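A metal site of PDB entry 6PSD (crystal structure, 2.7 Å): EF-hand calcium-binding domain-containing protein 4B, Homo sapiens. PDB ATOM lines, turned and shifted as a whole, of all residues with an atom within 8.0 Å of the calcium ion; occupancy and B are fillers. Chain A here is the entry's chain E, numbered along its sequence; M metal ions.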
ATOM      1  N   PHE A  24      20.075  10.358 -34.692  1.00  0.00           N
ATOM      2  CA  PHE A  24      20.627  10.021 -33.375  1.00  0.00           C
ATOM      3  C   PHE A  24      19.483   9.737 -32.449  1.00  0.00           C
ATOM      4  O   PHE A  24      18.344  10.032 -32.780  1.00  0.00           O
ATOM      5  CB  PHE A  24      21.491  11.121 -32.833  1.00  0.00           C
ATOM      6  CG  PHE A  24      20.752  12.396 -32.569  1.00  0.00           C
ATOM      7  CD1 PHE A  24      20.675  13.393 -33.552  1.00  0.00           C
ATOM      8  CD2 PHE A  24      20.194  12.620 -31.331  1.00  0.00           C
ATOM      9  CE1 PHE A  24      20.045  14.606 -33.282  1.00  0.00           C
ATOM     10  CE2 PHE A  24      19.549  13.814 -31.066  1.00  0.00           C
ATOM     11  CZ  PHE A  24      19.489  14.813 -32.026  1.00  0.00           C
ATOM     12  N   ILE A  25      19.801   9.151 -31.306  1.00  0.00           N
ATOM     13  CA  ILE A  25      18.787   8.787 -30.309  1.00  0.00           C
ATOM     14  C   ILE A  25      18.971   9.717 -29.130  1.00  0.00           C
ATOM     15  O   ILE A  25      20.069   9.821 -28.590  1.00  0.00           O
ATOM     16  CB  ILE A  25      18.854   7.321 -29.861  1.00  0.00           C
ATOM     17  CG1 ILE A  25      18.603   6.364 -31.059  1.00  0.00           C
ATOM     18  CG2 ILE A  25      17.819   7.027 -28.821  1.00  0.00           C
ATOM     19  CD1 ILE A  25      19.282   5.025 -30.921  1.00  0.00           C
ATOM     20  N   PHE A  48      20.142   3.805 -21.817  1.00  0.00           N
ATOM     21  CA  PHE A  48      20.649   4.961 -22.451  1.00  0.00           C
ATOM     22  C   PHE A  48      22.001   5.274 -21.915  1.00  0.00           C
ATOM     23  O   PHE A  48      22.918   5.495 -22.634  1.00  0.00           O
ATOM     24  CB  PHE A  48      19.765   6.156 -22.214  1.00  0.00           C
ATOM     25  CG  PHE A  48      20.091   7.301 -23.093  1.00  0.00           C
ATOM     26  CD1 PHE A  48      21.195   8.058 -22.859  1.00  0.00           C
ATOM     27  CD2 PHE A  48      19.329   7.594 -24.164  1.00  0.00           C
ATOM     28  CE1 PHE A  48      21.514   9.110 -23.689  1.00  0.00           C
ATOM     29  CE2 PHE A  48      19.653   8.642 -24.970  1.00  0.00           C
ATOM     30  CZ  PHE A  48      20.741   9.385 -24.732  1.00  0.00           C
ATOM     31  N   LEU A  51      24.800   3.200 -22.982  1.00  0.00           N
ATOM     32  CA  LEU A  51      25.154   3.306 -24.393  1.00  0.00           C
ATOM     33  C   LEU A  51      25.798   4.622 -24.827  1.00  0.00           C
ATOM     34  O   LEU A  51      26.483   4.650 -25.841  1.00  0.00           O
ATOM     35  CB  LEU A  51      23.912   3.094 -25.275  1.00  0.00           C
ATOM     36  CG  LEU A  51      23.409   1.660 -25.494  1.00  0.00           C
ATOM     37  CD1 LEU A  51      22.159   1.682 -26.366  1.00  0.00           C
ATOM     38  CD2 LEU A  51      24.448   0.763 -26.111  1.00  0.00           C
ATOM     39  N   ASP A  52      25.598   5.713 -24.087  1.00  0.00           N
ATOM     40  CA  ASP A  52      26.245   6.966 -24.473  1.00  0.00           C
ATOM     41  C   ASP A  52      27.644   7.046 -23.878  1.00  0.00           C
ATOM     42  O   ASP A  52      27.855   7.598 -22.831  1.00  0.00           O
ATOM     43  CB  ASP A  52      25.398   8.194 -24.081  1.00  0.00           C
ATOM     44  CG  ASP A  52      25.846   9.451 -24.841  1.00  0.00           C
ATOM     45  OD1 ASP A  52      26.763   9.322 -25.674  1.00  0.00           O
ATOM     46  OD2 ASP A  52      25.248  10.546 -24.671  1.00  0.00           O
ATOM     47  N   ALA A  53      28.616   6.528 -24.607  1.00  0.00           N
ATOM     48  CA  ALA A  53      29.932   6.360 -24.059  1.00  0.00           C
ATOM     49  C   ALA A  53      30.554   7.674 -23.677  1.00  0.00           C
ATOM     50  O   ALA A  53      31.164   7.787 -22.641  1.00  0.00           O
ATOM     51  CB  ALA A  53      30.810   5.629 -25.058  1.00  0.00           C
ATOM     52  N   ASP A  54      30.373   8.686 -24.515  1.00  0.00           N
ATOM     53  CA  ASP A  54      30.969  10.018 -24.319  1.00  0.00           C
ATOM     54  C   ASP A  54      30.093  10.975 -23.501  1.00  0.00           C
ATOM     55  O   ASP A  54      30.499  12.121 -23.270  1.00  0.00           O
ATOM     56  CB  ASP A  54      31.305  10.663 -25.673  1.00  0.00           C
ATOM     57  CG  ASP A  54      30.066  10.925 -26.525  1.00  0.00           C
ATOM     58  OD1 ASP A  54      28.945  10.589 -26.076  1.00  0.00           O
ATOM     59  OD2 ASP A  54      30.199  11.460 -27.650  1.00  0.00           O
ATOM     60  N   GLY A  55      28.902  10.547 -23.097  1.00  0.00           N
ATOM     61  CA  GLY A  55      28.075  11.387 -22.269  1.00  0.00           C
ATOM     62  C   GLY A  55      27.572  12.661 -22.915  1.00  0.00           C
ATOM     63  O   GLY A  55      27.326  13.593 -22.222  1.00  0.00           O
ATOM     64  N   ASN A  56      27.357  12.658 -24.225  1.00  0.00           N
ATOM     65  CA  ASN A  56      26.711  13.802 -24.877  1.00  0.00           C
ATOM     66  C   ASN A  56      25.244  14.025 -24.495  1.00  0.00           C
ATOM     67  O   ASN A  56      24.687  15.055 -24.849  1.00  0.00           O
ATOM     68  CB  ASN A  56      26.777  13.634 -26.402  1.00  0.00           C
ATOM     69  CG  ASN A  56      28.160  13.644 -26.913  1.00  0.00           C
ATOM     70  OD1 ASN A  56      28.458  12.972 -27.916  1.00  0.00           O
ATOM     71  ND2 ASN A  56      29.048  14.371 -26.255  1.00  0.00           N
ATOM     72  N   GLY A  57      24.606  13.067 -23.828  1.00  0.00           N
ATOM     73  CA  GLY A  57      23.147  12.987 -23.852  1.00  0.00           C
ATOM     74  C   GLY A  57      22.584  12.712 -25.241  1.00  0.00           C
ATOM     75  O   GLY A  57      21.392  12.908 -25.470  1.00  0.00           O
ATOM     76  N   TYR A  58      23.419  12.234 -26.155  1.00  0.00           N
ATOM     77  CA  TYR A  58      23.051  11.981 -27.530  1.00  0.00           C
ATOM     78  C   TYR A  58      23.594  10.632 -27.916  1.00  0.00           C
ATOM     79  O   TYR A  58      24.812  10.384 -27.771  1.00  0.00           O
ATOM     80  CB  TYR A  58      23.599  13.057 -28.486  1.00  0.00           C
ATOM     81  CG  TYR A  58      23.005  14.425 -28.310  1.00  0.00           C
ATOM     82  CD1 TYR A  58      21.685  14.669 -28.661  1.00  0.00           C
ATOM     83  CD2 TYR A  58      23.758  15.468 -27.822  1.00  0.00           C
ATOM     84  CE1 TYR A  58      21.139  15.942 -28.538  1.00  0.00           C
ATOM     85  CE2 TYR A  58      23.221  16.730 -27.660  1.00  0.00           C
ATOM     86  CZ  TYR A  58      21.903  16.966 -28.029  1.00  0.00           C
ATOM     87  OH  TYR A  58      21.363  18.198 -27.889  1.00  0.00           O
ATOM     88  N   LEU A  59      22.723   9.769 -28.406  1.00  0.00           N
ATOM     89  CA  LEU A  59      23.116   8.414 -28.840  1.00  0.00           C
ATOM     90  C   LEU A  59      23.330   8.364 -30.354  1.00  0.00           C
ATOM     91  O   LEU A  59      22.400   8.570 -31.135  1.00  0.00           O
ATOM     92  CB  LEU A  59      22.077   7.385 -28.462  1.00  0.00           C
ATOM     93  CG  LEU A  59      22.527   6.453 -27.354  1.00  0.00           C
ATOM     94  CD1 LEU A  59      21.404   5.478 -27.008  1.00  0.00           C
ATOM     95  CD2 LEU A  59      23.794   5.728 -27.734  1.00  0.00           C
ATOM     96  N   THR A  60      24.571   8.148 -30.765  1.00  0.00           N
ATOM     97  CA  THR A  60      24.892   8.076 -32.170  1.00  0.00           C
ATOM     98  C   THR A  60      24.772   6.610 -32.692  1.00  0.00           C
ATOM     99  O   THR A  60      24.834   5.635 -31.938  1.00  0.00           O
ATOM    100  CB  THR A  60      26.300   8.573 -32.413  1.00  0.00           C
ATOM    101  OG1 THR A  60      27.201   7.927 -31.505  1.00  0.00           O
ATOM    102  CG2 THR A  60      26.416  10.108 -32.193  1.00  0.00           C
ATOM    103  N   PRO A  61      24.620   6.460 -33.998  1.00  0.00           N
ATOM    104  CA  PRO A  61      24.639   5.107 -34.563  1.00  0.00           C
ATOM    105  C   PRO A  61      25.849   4.284 -34.145  1.00  0.00           C
ATOM    106  O   PRO A  61      25.695   3.132 -33.777  1.00  0.00           O
ATOM    107  CB  PRO A  61      24.650   5.368 -36.056  1.00  0.00           C
ATOM    108  CG  PRO A  61      24.001   6.704 -36.232  1.00  0.00           C
ATOM    109  CD  PRO A  61      24.326   7.494 -35.011  1.00  0.00           C
ATOM    110  N   GLN A  62      27.040   4.860 -34.185  1.00  0.00           N
ATOM    111  CA  GLN A  62      28.251   4.162 -33.797  1.00  0.00           C
ATOM    112  C   GLN A  62      28.264   3.790 -32.363  1.00  0.00           C
ATOM    113  O   GLN A  62      28.789   2.771 -32.040  1.00  0.00           O
ATOM    114  CB  GLN A  62      29.538   4.862 -34.227  1.00  0.00           C
ATOM    115  CG  GLN A  62      29.842   6.244 -33.681  1.00  0.00           C
ATOM    116  CD  GLN A  62      29.250   7.371 -34.538  1.00  0.00           C
ATOM    117  OE1 GLN A  62      28.180   7.206 -35.180  1.00  0.00           O
ATOM    118  NE2 GLN A  62      29.931   8.521 -34.561  1.00  0.00           N
ATOM    119  N   GLU A  63      27.702   4.608 -31.506  1.00  0.00           N
ATOM    120  CA  GLU A  63      27.548   4.297 -30.107  1.00  0.00           C
ATOM    121  C   GLU A  63      26.493   3.212 -29.957  1.00  0.00           C
ATOM    122  O   GLU A  63      26.652   2.292 -29.139  1.00  0.00           O
ATOM    123  CB  GLU A  63      27.124   5.535 -29.322  1.00  0.00           C
ATOM    124  CG  GLU A  63      28.262   6.516 -29.004  1.00  0.00           C
ATOM    125  CD  GLU A  63      27.775   7.796 -28.353  1.00  0.00           C
ATOM    126  OE1 GLU A  63      28.535   8.285 -27.490  1.00  0.00           O
ATOM    127  OE2 GLU A  63      26.650   8.283 -28.643  1.00  0.00           O
ATOM    128  N   PHE A  64      25.410   3.315 -30.714  1.00  0.00           N
ATOM    129  CA  PHE A  64      24.385   2.277 -30.679  1.00  0.00           C
ATOM    130  C   PHE A  64      24.926   0.938 -31.222  1.00  0.00           C
ATOM    131  O   PHE A  64      24.763  -0.099 -30.588  1.00  0.00           O
ATOM    132  CB  PHE A  64      23.208   2.722 -31.524  1.00  0.00           C
ATOM    133  CG  PHE A  64      21.997   1.860 -31.388  1.00  0.00           C
ATOM    134  CD1 PHE A  64      21.087   2.087 -30.376  1.00  0.00           C
ATOM    135  CD2 PHE A  64      21.777   0.834 -32.258  1.00  0.00           C
ATOM    136  CE1 PHE A  64      19.965   1.334 -30.254  1.00  0.00           C
ATOM    137  CE2 PHE A  64      20.638   0.046 -32.156  1.00  0.00           C
ATOM    138  CZ  PHE A  64      19.705   0.314 -31.176  1.00  0.00           C
HETATM  139 CA    CA M   1      27.104  10.371 -27.547  1.00  0.00          CA
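OD2 of Asp 52 sits at hydrogen-bond distance from N of Asn 56, 3.0 Å away. The side-chain carboxylate of Asp 52 sits at hydrogen-bond distance from the backbone NH of Gly 57. ND2 of Asn 56 lies close to OD2 of Asp 54 (3.4 Å). The backbone NH (N) of Glu 63 sits close to the side-chain hydroxyl (OG1) of Thr 60, 3.4 Å away. OE1 of Glu 63 lies close to N of Ala 53 (3.4 Å).
Within 4 Å of the calcium ion: Asp 52, Asp 54, Asn 56, Tyr 58 and Glu 63. The nearest printed residue that does not touch the calcium ion is Leu 59 (4.5 Å).
The calcium ion is bound by OD1 of Asp 52 (2.2 Å), O of Tyr 58 (2.3 Å), OD1 of Asp 54 (2.4 Å), OE2 of Glu 63 (2.4 Å) and OE1 of Glu 63 (2.5 Å). Slightly farther from the calcium ion lies the side-chain amide oxygen (OD1) of Asn 56 (3.0 Å).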
